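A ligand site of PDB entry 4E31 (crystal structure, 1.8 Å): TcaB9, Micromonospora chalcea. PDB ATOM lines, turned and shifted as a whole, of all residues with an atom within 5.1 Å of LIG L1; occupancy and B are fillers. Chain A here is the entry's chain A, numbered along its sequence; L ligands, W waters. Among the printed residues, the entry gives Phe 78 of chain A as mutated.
ND2 of Asn 117 lies within hydrogen-bond range of O of Tyr 80 (2.9 Å).
The side-chain carboxylate (OE2) of Glu 136 sits at hydrogen-bond distance from the backbone NH (N) of Ser 138, 2.8 Å away.
The backbone carbonyl oxygen (O) of Ala 178 lies within hydrogen-bond range of the side-chain hydroxyl (OG1) of Thr 180 (2.9 Å).
N of Asn 117 lies within hydrogen-bond range of OE1 of Glu 136, at 2.8 Å.
O of Asn 179 lies close to NE2 of His 183.
The backbone NH (N) of Phe 135 sits at hydrogen-bond distance from the backbone carbonyl oxygen (O) of Glu 113.
OH of Tyr 186 lies within hydrogen-bond range of NH1 of Arg 70, at 3.0 Å.
The backbone NH (N) of Gly 115 sits at hydrogen-bond distance from the backbone carbonyl oxygen (O) of Phe 135, at 2.8 Å.
CD1 of Phe 74 touches C8 of LIG L1, 3.6 Å away.
CE2 of Phe 78 touches O4 of LIG L1 (3.5 Å).
Tyr 80 touches LIG L1 (CE2 to O2, 3.99 Å).
Phe 92 touches LIG L1.
Ile 114 touches LIG L1 (CG2 to C13, 3.4 Å).
O of Phe 135 touches N6 of LIG L1, 3.6 Å away.
Pro 137 touches LIG L1 (CD to N6, 3.2 Å).
CB of Phe 156 touches N4 of LIG L1, at 3.6 Å.
CD1 of Ile 184 touches N4 of LIG L1, at 3.5 Å.
OG of Ser 138 sits at hydrogen-bond distance from O5 of LIG L1, 2.8 Å away.
A nitrogen (N1) of LIG L1 lies within salt-bridge range of the side-chain carboxylate (OE1) of Glu 113, at 3.8 Å.
ND2 of Asn 117 is in hydrogen-bond range of O4 of LIG L1 (3.4 Å).
A nitrogen (N1) of LG2 L2 sits at hydrogen-bond distance from a ring nitrogen (NE2) of His 183 (2.9 Å).
The backbone carbonyl oxygen of Gly 115 is in hydrogen-bond range of a nitrogen (N1) of LIG L1, 2.9 Å away.
The backbone carbonyl oxygen (O) of Ala 178 lies within hydrogen-bond range of a nitrogen (N1) of LIG L1 (3.1 Å).
N of Phe 157 sits at hydrogen-bond distance from N5 of LIG L1, 2.9 Å away.
The backbone carbonyl oxygen of Phe 157 sits at hydrogen-bond distance from a nitrogen (N4) of LIG L1 (3.2 Å).
A nitrogen (N4) of LIG L1 sits at hydrogen-bond distance from the side-chain hydroxyl (OH) of Tyr 186 (2.9 Å).
The side-chain amide nitrogen of Asn 179 is in hydrogen-bond range of an oxygen (O1) of LIG L1, 2.9 Å away.
O2 of LIG L1 sits at hydrogen-bond distance from OG of Ser 82 (2.8 Å).
The side-chain carboxylate (OE1) of Glu 136 is in hydrogen-bond range of an oxygen (O4) of LIG L1.
N6 of LIG L1 lies within hydrogen-bond range of N of Gly 115, at 3.2 Å.
The side-chain hydroxyl of Tyr 80 sits at hydrogen-bond distance from an oxygen (O4) of LG2 L2, at 2.7 Å.
OG1 of Thr 180 sits close to O3 of LIG L1, 3.4 Å away.
Water W1 lies within hydrogen-bond range of O2 of LIG L1 (2.6 Å), NE2 of His 256 (2.8 Å) and OH of Tyr 80 (3.4 Å).
Water W3 bridges the side-chain carboxylate of Glu 113 (2.7 Å) and a nitrogen (N1) of LIG L1 (2.7 Å).
Water W2 lies within hydrogen-bond range of OH of Tyr 186 (2.6 Å) and N3 of LIG L1 (2.9 Å).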
ATOM      1  N   ARG A  70      -5.104   9.541 -32.540  1.00  0.00           N
ATOM      2  CA  ARG A  70      -4.416   9.865 -31.289  1.00  0.00           C
ATOM      3  C   ARG A  70      -5.153  10.884 -30.422  1.00  0.00           C
ATOM      4  O   ARG A  70      -5.149  10.834 -29.186  1.00  0.00           O
ATOM      5  CB  ARG A  70      -3.000  10.331 -31.582  1.00  0.00           C
ATOM      6  CG  ARG A  70      -2.915  11.573 -32.488  1.00  0.00           C
ATOM      7  CD  ARG A  70      -1.447  11.839 -32.752  1.00  0.00           C
ATOM      8  NE  ARG A  70      -1.201  13.117 -33.435  1.00  0.00           N
ATOM      9  CZ  ARG A  70      -0.002  13.538 -33.831  1.00  0.00           C
ATOM     10  NH1 ARG A  70       1.087  12.810 -33.583  1.00  0.00           N
ATOM     11  NH2 ARG A  70       0.149  14.718 -34.443  1.00  0.00           N
ATOM     12  N   PHE A  74      -5.399  10.762 -26.276  1.00  0.00           N
ATOM     13  CA  PHE A  74      -4.442  11.550 -25.512  1.00  0.00           C
ATOM     14  C   PHE A  74      -4.747  13.041 -25.721  1.00  0.00           C
ATOM     15  O   PHE A  74      -4.672  13.540 -26.855  1.00  0.00           O
ATOM     16  CB  PHE A  74      -3.089  11.159 -26.095  1.00  0.00           C
ATOM     17  CG  PHE A  74      -2.849   9.670 -26.177  1.00  0.00           C
ATOM     18  CD1 PHE A  74      -2.864   8.912 -25.017  1.00  0.00           C
ATOM     19  CD2 PHE A  74      -2.601   9.052 -27.413  1.00  0.00           C
ATOM     20  CE1 PHE A  74      -2.649   7.536 -25.047  1.00  0.00           C
ATOM     21  CE2 PHE A  74      -2.376   7.667 -27.460  1.00  0.00           C
ATOM     22  CZ  PHE A  74      -2.408   6.941 -26.282  1.00  0.00           C
ATOM     23  N   PHE A  78      -7.009  12.904 -20.557  1.00  0.00           N
ATOM     24  CA  PHE A  78      -6.468  11.570 -20.450  1.00  0.00           C
ATOM     25  C   PHE A  78      -6.136  11.390 -18.950  1.00  0.00           C
ATOM     26  O   PHE A  78      -5.463  12.227 -18.326  1.00  0.00           O
ATOM     27  CB  PHE A  78      -5.218  11.486 -21.330  1.00  0.00           C
ATOM     28  CG  PHE A  78      -4.422  10.233 -21.058  1.00  0.00           C
ATOM     29  CD1 PHE A  78      -4.780   9.030 -21.648  1.00  0.00           C
ATOM     30  CD2 PHE A  78      -3.292  10.282 -20.260  1.00  0.00           C
ATOM     31  CE1 PHE A  78      -4.036   7.847 -21.437  1.00  0.00           C
ATOM     32  CE2 PHE A  78      -2.517   9.120 -20.046  1.00  0.00           C
ATOM     33  CZ  PHE A  78      -2.895   7.907 -20.626  1.00  0.00           C
ATOM     34  N   TYR A  80      -4.672   8.835 -16.915  1.00  0.00           N
ATOM     35  CA  TYR A  80      -3.819   7.878 -16.187  1.00  0.00           C
ATOM     36  C   TYR A  80      -2.684   8.614 -15.471  1.00  0.00           C
ATOM     37  O   TYR A  80      -1.956   9.372 -16.136  1.00  0.00           O
ATOM     38  CB  TYR A  80      -3.159   6.894 -17.159  1.00  0.00           C
ATOM     39  CG  TYR A  80      -2.319   5.854 -16.460  1.00  0.00           C
ATOM     40  CD1 TYR A  80      -2.875   4.884 -15.641  1.00  0.00           C
ATOM     41  CD2 TYR A  80      -0.916   5.873 -16.615  1.00  0.00           C
ATOM     42  CE1 TYR A  80      -2.076   3.953 -14.983  1.00  0.00           C
ATOM     43  CE2 TYR A  80      -0.113   4.957 -15.974  1.00  0.00           C
ATOM     44  CZ  TYR A  80      -0.710   4.006 -15.166  1.00  0.00           C
ATOM     45  OH  TYR A  80       0.093   3.052 -14.602  1.00  0.00           O
ATOM     46  N   SER A  82       0.733   7.945 -13.732  1.00  0.00           N
ATOM     47  CA  SER A  82       1.732   6.907 -13.519  1.00  0.00           C
ATOM     48  C   SER A  82       2.132   6.776 -12.042  1.00  0.00           C
ATOM     49  O   SER A  82       2.372   5.671 -11.567  1.00  0.00           O
ATOM     50  CB  SER A  82       2.976   7.344 -14.284  1.00  0.00           C
ATOM     51  OG  SER A  82       2.649   7.396 -15.665  1.00  0.00           O
ATOM     52  N   PHE A  92      10.818   3.453 -11.947  1.00  0.00           N
ATOM     53  CA  PHE A  92      11.364   4.494 -12.802  1.00  0.00           C
ATOM     54  C   PHE A  92      12.493   5.327 -12.179  1.00  0.00           C
ATOM     55  O   PHE A  92      13.414   5.729 -12.882  1.00  0.00           O
ATOM     56  CB  PHE A  92      10.245   5.419 -13.316  1.00  0.00           C
ATOM     57  CG  PHE A  92       9.339   4.728 -14.287  1.00  0.00           C
ATOM     58  CD1 PHE A  92       9.825   4.340 -15.533  1.00  0.00           C
ATOM     59  CD2 PHE A  92       8.004   4.473 -13.960  1.00  0.00           C
ATOM     60  CE1 PHE A  92       9.047   3.687 -16.473  1.00  0.00           C
ATOM     61  CE2 PHE A  92       7.195   3.850 -14.899  1.00  0.00           C
ATOM     62  CZ  PHE A  92       7.715   3.424 -16.158  1.00  0.00           C
ATOM     63  N   GLU A 113      12.284  12.224 -22.817  1.00  0.00           N
ATOM     64  CA  GLU A 113      11.390  11.101 -22.565  1.00  0.00           C
ATOM     65  C   GLU A 113      10.152  11.355 -23.399  1.00  0.00           C
ATOM     66  O   GLU A 113       9.642  12.466 -23.392  1.00  0.00           O
ATOM     67  CB  GLU A 113      10.943  11.073 -21.095  1.00  0.00           C
ATOM     68  CG  GLU A 113      10.014   9.895 -20.877  1.00  0.00           C
ATOM     69  CD  GLU A 113       9.716   9.585 -19.409  1.00  0.00           C
ATOM     70  OE1 GLU A 113       9.247   8.457 -19.130  1.00  0.00           O
ATOM     71  OE2 GLU A 113       9.947  10.464 -18.544  1.00  0.00           O
ATOM     72  N   ILE A 114       9.640  10.300 -24.043  1.00  0.00           N
ATOM     73  CA  ILE A 114       8.439  10.331 -24.879  1.00  0.00           C
ATOM     74  C   ILE A 114       7.404   9.758 -23.930  1.00  0.00           C
ATOM     75  O   ILE A 114       7.515   8.597 -23.516  1.00  0.00           O
ATOM     76  CB  ILE A 114       8.595   9.452 -26.129  1.00  0.00           C
ATOM     77  CG1 ILE A 114       9.801   9.883 -26.965  1.00  0.00           C
ATOM     78  CG2 ILE A 114       7.276   9.404 -26.952  1.00  0.00           C
ATOM     79  CD1 ILE A 114      10.087   9.103 -28.239  1.00  0.00           C
ATOM     80  N   GLY A 115       6.379  10.546 -23.639  1.00  0.00           N
ATOM     81  CA  GLY A 115       5.335  10.045 -22.744  1.00  0.00           C
ATOM     82  C   GLY A 115       5.658  10.207 -21.274  1.00  0.00           C
ATOM     83  O   GLY A 115       5.432   9.298 -20.479  1.00  0.00           O
ATOM     84  N   CYS A 116       6.176  11.365 -20.849  1.00  0.00           N
ATOM     85  CA  CYS A 116       6.634  11.424 -19.456  1.00  0.00           C
ATOM     86  C   CYS A 116       5.488  11.469 -18.430  1.00  0.00           C
ATOM     87  O   CYS A 116       5.762  11.299 -17.233  1.00  0.00           O
ATOM     88  CB  CYS A 116       7.568  12.634 -19.249  1.00  0.00           C
ATOM     89  SG  CYS A 116       6.715  14.260 -19.487  1.00  0.00           S
ATOM     90  N   ASN A 117       4.246  11.658 -18.875  1.00  0.00           N
ATOM     91  CA  ASN A 117       3.102  11.668 -17.962  1.00  0.00           C
ATOM     92  C   ASN A 117       3.348  12.653 -16.823  1.00  0.00           C
ATOM     93  O   ASN A 117       3.771  13.785 -17.081  1.00  0.00           O
ATOM     94  CB  ASN A 117       2.885  10.216 -17.504  1.00  0.00           C
ATOM     95  CG  ASN A 117       1.517   9.988 -16.840  1.00  0.00           C
ATOM     96  OD1 ASN A 117       1.366  10.083 -15.623  1.00  0.00           O
ATOM     97  ND2 ASN A 117       0.512   9.665 -17.657  1.00  0.00           N
ATOM     98  N   ILE A 120       7.026  10.826 -13.401  1.00  0.00           N
ATOM     99  CA  ILE A 120       7.458   9.656 -12.645  1.00  0.00           C
ATOM    100  C   ILE A 120       8.951   9.327 -12.883  1.00  0.00           C
ATOM    101  O   ILE A 120       9.615   8.894 -11.931  1.00  0.00           O
ATOM    102  CB  ILE A 120       6.513   8.446 -12.904  1.00  0.00           C
ATOM    103  CG1 ILE A 120       6.789   7.313 -11.903  1.00  0.00           C
ATOM    104  CG2 ILE A 120       6.497   7.921 -14.352  1.00  0.00           C
ATOM    105  CD1 ILE A 120       5.703   6.215 -11.882  1.00  0.00           C
ATOM    106  N   PHE A 135       8.121  14.912 -23.584  1.00  0.00           N
ATOM    107  CA  PHE A 135       6.977  15.073 -24.485  1.00  0.00           C
ATOM    108  C   PHE A 135       5.760  14.464 -23.788  1.00  0.00           C
ATOM    109  O   PHE A 135       5.782  13.284 -23.390  1.00  0.00           O
ATOM    110  CB  PHE A 135       7.239  14.300 -25.776  1.00  0.00           C
ATOM    111  CG  PHE A 135       8.073  15.102 -26.711  1.00  0.00           C
ATOM    112  CD1 PHE A 135       7.481  15.897 -27.671  1.00  0.00           C
ATOM    113  CD2 PHE A 135       9.468  15.094 -26.585  1.00  0.00           C
ATOM    114  CE1 PHE A 135       8.274  16.647 -28.542  1.00  0.00           C
ATOM    115  CE2 PHE A 135      10.272  15.854 -27.443  1.00  0.00           C
ATOM    116  CZ  PHE A 135       9.666  16.626 -28.434  1.00  0.00           C
ATOM    117  N   GLU A 136       4.715  15.276 -23.658  1.00  0.00           N
ATOM    118  CA  GLU A 136       3.528  14.777 -22.954  1.00  0.00           C
ATOM    119  C   GLU A 136       2.364  15.580 -23.547  1.00  0.00           C
ATOM    120  O   GLU A 136       2.061  16.675 -23.075  1.00  0.00           O
ATOM    121  CB  GLU A 136       3.640  14.897 -21.436  1.00  0.00           C
ATOM    122  CG  GLU A 136       2.455  14.289 -20.658  1.00  0.00           C
ATOM    123  CD  GLU A 136       1.989  13.021 -21.366  1.00  0.00           C
ATOM    124  OE1 GLU A 136       2.579  11.952 -21.055  1.00  0.00           O
ATOM    125  OE2 GLU A 136       1.065  13.060 -22.214  1.00  0.00           O
ATOM    126  N   PRO A 137       1.691  14.984 -24.549  1.00  0.00           N
ATOM    127  CA  PRO A 137       0.635  15.708 -25.247  1.00  0.00           C
ATOM    128  C   PRO A 137      -0.669  15.680 -24.446  1.00  0.00           C
ATOM    129  O   PRO A 137      -1.621  16.291 -24.905  1.00  0.00           O
ATOM    130  CB  PRO A 137       0.448  14.886 -26.530  1.00  0.00           C
ATOM    131  CG  PRO A 137       0.775  13.458 -26.078  1.00  0.00           C
ATOM    132  CD  PRO A 137       1.995  13.706 -25.212  1.00  0.00           C
ATOM    133  N   SER A 138      -0.709  14.988 -23.306  1.00  0.00           N
ATOM    134  CA  SER A 138      -1.932  15.010 -22.476  1.00  0.00           C
ATOM    135  C   SER A 138      -1.691  16.052 -21.380  1.00  0.00           C
ATOM    136  O   SER A 138      -0.932  15.815 -20.441  1.00  0.00           O
ATOM    137  CB  SER A 138      -2.258  13.636 -21.878  1.00  0.00           C
ATOM    138  OG  SER A 138      -2.547  12.674 -22.889  1.00  0.00           O
ATOM    139  N   VAL A 141      -1.820  15.626 -17.221  1.00  0.00           N
ATOM    140  CA  VAL A 141      -0.657  15.031 -16.568  1.00  0.00           C
ATOM    141  C   VAL A 141       0.614  15.823 -16.868  1.00  0.00           C
ATOM    142  O   VAL A 141       1.504  15.939 -16.011  1.00  0.00           O
ATOM    143  CB  VAL A 141      -0.530  13.514 -16.842  1.00  0.00           C
ATOM    144  CG1 VAL A 141      -1.789  12.849 -16.313  1.00  0.00           C
ATOM    145  CG2 VAL A 141      -0.388  13.289 -18.351  1.00  0.00           C
ATOM    146  N   ASP A 155       3.189  18.152 -26.509  1.00  0.00           N
ATOM    147  CA  ASP A 155       3.105  17.797 -27.931  1.00  0.00           C
ATOM    148  C   ASP A 155       3.351  16.307 -28.112  1.00  0.00           C
ATOM    149  O   ASP A 155       3.944  15.665 -27.251  1.00  0.00           O
ATOM    150  CB  ASP A 155       4.310  18.375 -28.670  1.00  0.00           C
ATOM    151  CG  ASP A 155       4.051  19.781 -29.178  1.00  0.00           C
ATOM    152  OD1 ASP A 155       4.829  20.679 -28.760  1.00  0.00           O
ATOM    153  OD2 ASP A 155       3.097  19.950 -29.984  1.00  0.00           O
ATOM    154  N   PHE A 156       2.911  15.768 -29.240  1.00  0.00           N
ATOM    155  CA  PHE A 156       3.324  14.429 -29.584  1.00  0.00           C
ATOM    156  C   PHE A 156       4.766  14.457 -30.096  1.00  0.00           C
ATOM    157  O   PHE A 156       5.171  15.373 -30.832  1.00  0.00           O
ATOM    158  CB  PHE A 156       2.388  13.872 -30.657  1.00  0.00           C
ATOM    159  CG  PHE A 156       0.930  13.750 -30.210  1.00  0.00           C
ATOM    160  CD1 PHE A 156       0.536  12.615 -29.518  1.00  0.00           C
ATOM    161  CD2 PHE A 156      -0.035  14.713 -30.513  1.00  0.00           C
ATOM    162  CE1 PHE A 156      -0.787  12.429 -29.087  1.00  0.00           C
ATOM    163  CE2 PHE A 156      -1.372  14.554 -30.093  1.00  0.00           C
ATOM    164  CZ  PHE A 156      -1.747  13.397 -29.384  1.00  0.00           C
ATOM    165  N   PHE A 157       5.555  13.473 -29.668  1.00  0.00           N
ATOM    166  CA  PHE A 157       6.826  13.183 -30.328  1.00  0.00           C
ATOM    167  C   PHE A 157       6.519  12.583 -31.693  1.00  0.00           C
ATOM    168  O   PHE A 157       5.754  11.619 -31.768  1.00  0.00           O
ATOM    169  CB  PHE A 157       7.622  12.195 -29.478  1.00  0.00           C
ATOM    170  CG  PHE A 157       9.044  12.040 -29.927  1.00  0.00           C
ATOM    171  CD1 PHE A 157       9.357  11.161 -30.951  1.00  0.00           C
ATOM    172  CD2 PHE A 157      10.046  12.808 -29.359  1.00  0.00           C
ATOM    173  CE1 PHE A 157      10.662  10.979 -31.418  1.00  0.00           C
ATOM    174  CE2 PHE A 157      11.353  12.649 -29.830  1.00  0.00           C
ATOM    175  CZ  PHE A 157      11.655  11.748 -30.827  1.00  0.00           C
ATOM    176  N   ALA A 178       8.427   4.714 -22.063  1.00  0.00           N
ATOM    177  CA  ALA A 178       7.954   3.557 -21.299  1.00  0.00           C
ATOM    178  C   ALA A 178       6.429   3.517 -21.492  1.00  0.00           C
ATOM    179  O   ALA A 178       5.786   4.539 -21.293  1.00  0.00           O
ATOM    180  CB  ALA A 178       8.300   3.622 -19.782  1.00  0.00           C
ATOM    181  N   ASN A 179       5.868   2.375 -21.877  1.00  0.00           N
ATOM    182  CA  ASN A 179       4.413   2.284 -22.041  1.00  0.00           C
ATOM    183  C   ASN A 179       3.883   3.389 -22.956  1.00  0.00           C
ATOM    184  O   ASN A 179       2.825   3.943 -22.658  1.00  0.00           O
ATOM    185  CB  ASN A 179       3.697   2.299 -20.689  1.00  0.00           C
ATOM    186  CG  ASN A 179       4.324   1.250 -19.796  1.00  0.00           C
ATOM    187  OD1 ASN A 179       4.208   0.094 -20.212  1.00  0.00           O
ATOM    188  ND2 ASN A 179       5.040   1.587 -18.723  1.00  0.00           N
ATOM    189  N   THR A 180       4.696   3.732 -23.957  1.00  0.00           N
ATOM    190  CA  THR A 180       4.270   4.784 -24.917  1.00  0.00           C
ATOM    191  C   THR A 180       4.571   4.364 -26.352  1.00  0.00           C
ATOM    192  O   THR A 180       3.762   4.641 -27.250  1.00  0.00           O
ATOM    193  CB  THR A 180       5.033   6.109 -24.565  1.00  0.00           C
ATOM    194  OG1 THR A 180       4.706   6.485 -23.226  1.00  0.00           O
ATOM    195  CG2 THR A 180       4.451   7.232 -25.416  1.00  0.00           C
ATOM    196  N   HIS A 183       1.999   2.460 -28.194  1.00  0.00           N
ATOM    197  CA  HIS A 183       0.711   3.183 -28.264  1.00  0.00           C
ATOM    198  C   HIS A 183       0.644   4.004 -29.562  1.00  0.00           C
ATOM    199  O   HIS A 183      -0.396   4.612 -29.862  1.00  0.00           O
ATOM    200  CB  HIS A 183       0.602   4.245 -27.162  1.00  0.00           C
ATOM    201  CG  HIS A 183       0.491   3.664 -25.786  1.00  0.00           C
ATOM    202  ND1 HIS A 183       1.214   2.565 -25.344  1.00  0.00           N
ATOM    203  CD2 HIS A 183      -0.353   3.983 -24.783  1.00  0.00           C
ATOM    204  CE1 HIS A 183       0.828   2.274 -24.115  1.00  0.00           C
ATOM    205  NE2 HIS A 183      -0.097   3.139 -23.740  1.00  0.00           N
ATOM    206  N   ILE A 184       1.727   4.029 -30.324  1.00  0.00           N
ATOM    207  CA  ILE A 184       1.915   4.881 -31.495  1.00  0.00           C
ATOM    208  C   ILE A 184       1.950   4.143 -32.821  1.00  0.00           C
ATOM    209  O   ILE A 184       3.007   3.599 -33.142  1.00  0.00           O
ATOM    210  CB  ILE A 184       3.222   5.696 -31.358  1.00  0.00           C
ATOM    211  CG1 ILE A 184       3.103   6.604 -30.134  1.00  0.00           C
ATOM    212  CG2 ILE A 184       3.511   6.591 -32.574  1.00  0.00           C
ATOM    213  CD1 ILE A 184       4.412   7.209 -29.553  1.00  0.00           C
ATOM    214  N   TYR A 186       2.216   5.339 -35.611  1.00  0.00           N
ATOM    215  CA  TYR A 186       3.072   6.111 -36.524  1.00  0.00           C
ATOM    216  C   TYR A 186       4.518   5.987 -36.108  1.00  0.00           C
ATOM    217  O   TYR A 186       5.276   6.974 -36.015  1.00  0.00           O
ATOM    218  CB  TYR A 186       2.627   7.573 -36.729  1.00  0.00           C
ATOM    219  CG  TYR A 186       2.316   8.307 -35.424  1.00  0.00           C
ATOM    220  CD1 TYR A 186       1.094   8.165 -34.773  1.00  0.00           C
ATOM    221  CD2 TYR A 186       3.274   9.160 -34.858  1.00  0.00           C
ATOM    222  CE1 TYR A 186       0.829   8.837 -33.598  1.00  0.00           C
ATOM    223  CE2 TYR A 186       3.034   9.848 -33.687  1.00  0.00           C
ATOM    224  CZ  TYR A 186       1.815   9.671 -33.055  1.00  0.00           C
ATOM    225  OH  TYR A 186       1.537  10.340 -31.899  1.00  0.00           O
ATOM    226  N   HIS A 256       3.663  -4.417 -15.189  1.00  0.00           N
ATOM    227  CA  HIS A 256       2.575  -4.288 -16.160  1.00  0.00           C
ATOM    228  C   HIS A 256       2.279  -5.629 -16.797  1.00  0.00           C
ATOM    229  O   HIS A 256       1.939  -5.675 -17.988  1.00  0.00           O
ATOM    230  CB  HIS A 256       2.844  -3.209 -17.214  1.00  0.00           C
ATOM    231  CG  HIS A 256       2.666  -1.830 -16.667  1.00  0.00           C
ATOM    232  ND1 HIS A 256       1.471  -1.391 -16.121  1.00  0.00           N
ATOM    233  CD2 HIS A 256       3.542  -0.795 -16.561  1.00  0.00           C
ATOM    234  CE1 HIS A 256       1.630  -0.153 -15.687  1.00  0.00           C
ATOM    235  NE2 HIS A 256       2.865   0.242 -15.951  1.00  0.00           N
HETATM  236  N1  LIG L   1       5.888   6.744 -19.170  1.00  0.00           N
HETATM  237  C1  LIG L   1       4.693   6.644 -18.278  1.00  0.00           C
HETATM  238  C2  LIG L   1       3.391   7.049 -18.948  1.00  0.00           C
HETATM  239  C3  LIG L   1       2.697   6.009 -19.824  1.00  0.00           C
HETATM  240  S1  LIG L   1       1.091   6.555 -20.317  1.00  0.00           S
HETATM  241  C4  LIG L   1       4.582   5.282 -17.641  1.00  0.00           C
HETATM  242  O1  LIG L   1       5.255   4.368 -18.116  1.00  0.00           O
HETATM  243  O2  LIG L   1       3.813   5.056 -16.683  1.00  0.00           O
HETATM  244  C5  LIG L   1       1.371   6.824 -22.049  1.00  0.00           C
HETATM  245  C6  LIG L   1       1.638   8.309 -22.249  1.00  0.00           C
HETATM  246  O3  LIG L   1       2.033   8.533 -23.603  1.00  0.00           O
HETATM  247  C7  LIG L   1       0.385   9.169 -22.025  1.00  0.00           C
HETATM  248  O4  LIG L   1       0.659  10.157 -21.006  1.00  0.00           O
HETATM  249  C8  LIG L   1       0.219   9.823 -23.395  1.00  0.00           C
HETATM  250  O5  LIG L   1      -0.279  11.157 -23.460  1.00  0.00           O
HETATM  251  C9  LIG L   1       1.636   9.847 -23.960  1.00  0.00           C
HETATM  252  N2  LIG L   1       1.712   9.844 -25.457  1.00  0.00           N
HETATM  253  C10 LIG L   1       0.928   9.297 -26.420  1.00  0.00           C
HETATM  254  N3  LIG L   1       1.414   9.468 -27.682  1.00  0.00           N
HETATM  255  C11 LIG L   1       2.563  10.173 -27.471  1.00  0.00           C
HETATM  256  C12 LIG L   1       3.603  10.720 -28.387  1.00  0.00           C
HETATM  257  N4  LIG L   1       3.497  10.591 -29.713  1.00  0.00           N
HETATM  258  N5  LIG L   1       4.616  11.389 -27.807  1.00  0.00           N
HETATM  259  C13 LIG L   1       4.697  11.553 -26.473  1.00  0.00           C
HETATM  260  N6  LIG L   1       3.856  11.084 -25.545  1.00  0.00           N
HETATM  261  C14 LIG L   1       2.776  10.396 -26.036  1.00  0.00           C
HETATM  262  P1  LG2 L   2      -2.555   0.305 -14.435  1.00  0.00           P
HETATM  263  C1  LG2 L   2      -2.892   2.619 -18.338  1.00  0.00           C
HETATM  264  O1  LG2 L   2      -3.147   1.202 -18.301  1.00  0.00           O
HETATM  265  C2  LG2 L   2      -3.189   3.112 -19.741  1.00  0.00           C
HETATM  266  P2  LG2 L   2      -3.948   0.674 -17.028  1.00  0.00           P
HETATM  267  C3  LG2 L   2      -1.967   3.011 -20.675  1.00  0.00           C
HETATM  268  N1  LG2 L   2      -2.418   2.728 -22.042  1.00  0.00           N
HETATM  269  C4  LG2 L   2      -0.922   2.042 -20.184  1.00  0.00           C
HETATM  270  O2  LG2 L   2      -0.314   1.218 -20.852  1.00  0.00           O
HETATM  271  C5  LG2 L   2      -0.607   2.016 -18.720  1.00  0.00           C
HETATM  272  O3  LG2 L   2      -1.520   2.813 -17.984  1.00  0.00           O
HETATM  273  C6  LG2 L   2       0.815   2.410 -18.375  1.00  0.00           C
HETATM  274  C7  LG2 L   2      -5.662   1.926  -9.755  1.00  0.00           C
HETATM  275  N2  LG2 L   2      -4.926   1.529  -8.550  1.00  0.00           N
HETATM  276  O4  LG2 L   2      -1.297   0.909 -13.857  1.00  0.00           O
HETATM  277  C8  LG2 L   2      -4.980   3.129 -10.410  1.00  0.00           C
HETATM  278  C9  LG2 L   2      -5.501   1.539  -7.331  1.00  0.00           C
HETATM  279  O5  LG2 L   2      -6.702   1.875  -7.244  1.00  0.00           O
HETATM  280  O6  LG2 L   2      -2.694  -1.217 -14.395  1.00  0.00           O
HETATM  281  C10 LG2 L   2      -5.210   2.980 -11.910  1.00  0.00           C
HETATM  282  O7  LG2 L   2      -6.515   3.483 -12.204  1.00  0.00           O
HETATM  283  N3  LG2 L   2      -4.808   1.161  -6.230  1.00  0.00           N
HETATM  284  C11 LG2 L   2      -1.216   4.344 -20.681  1.00  0.00           C
HETATM  285  O8  LG2 L   2      -4.256  -0.767 -17.365  1.00  0.00           O
HETATM  286  C12 LG2 L   2      -5.355   1.455 -11.986  1.00  0.00           C
HETATM  287  O9  LG2 L   2      -5.698   0.887 -10.734  1.00  0.00           O
HETATM  288  C13 LG2 L   2      -3.494   0.826  -6.243  1.00  0.00           C
HETATM  289  O10 LG2 L   2      -2.891   0.490  -5.195  1.00  0.00           O
HETATM  290  O11 LG2 L   2      -5.103   1.568 -16.619  1.00  0.00           O
HETATM  291  C14 LG2 L   2      -4.116   0.656 -12.392  1.00  0.00           C
HETATM  292  O12 LG2 L   2      -3.846   0.994 -13.749  1.00  0.00           O
HETATM  293  C15 LG2 L   2      -2.819   0.819  -7.568  1.00  0.00           C
HETATM  294  C16 LG2 L   2      -1.369   0.426  -7.777  1.00  0.00           C
HETATM  295  C17 LG2 L   2      -3.629   1.139  -8.660  1.00  0.00           C
HETATM  296  O13 LG2 L   2      -2.758   0.774 -15.946  1.00  0.00           O
HETATM  297  O   HOH W   1       3.425   2.865 -15.260  1.00  0.00           O
HETATM  298  O   HOH W   2      -0.120   9.242 -30.151  1.00  0.00           O
HETATM  299  O   HOH W   3       8.036   6.776 -17.467  1.00  0.00           O
HETATM  300  O   HOH W   4       7.867   7.250 -21.107  1.00  0.00           O
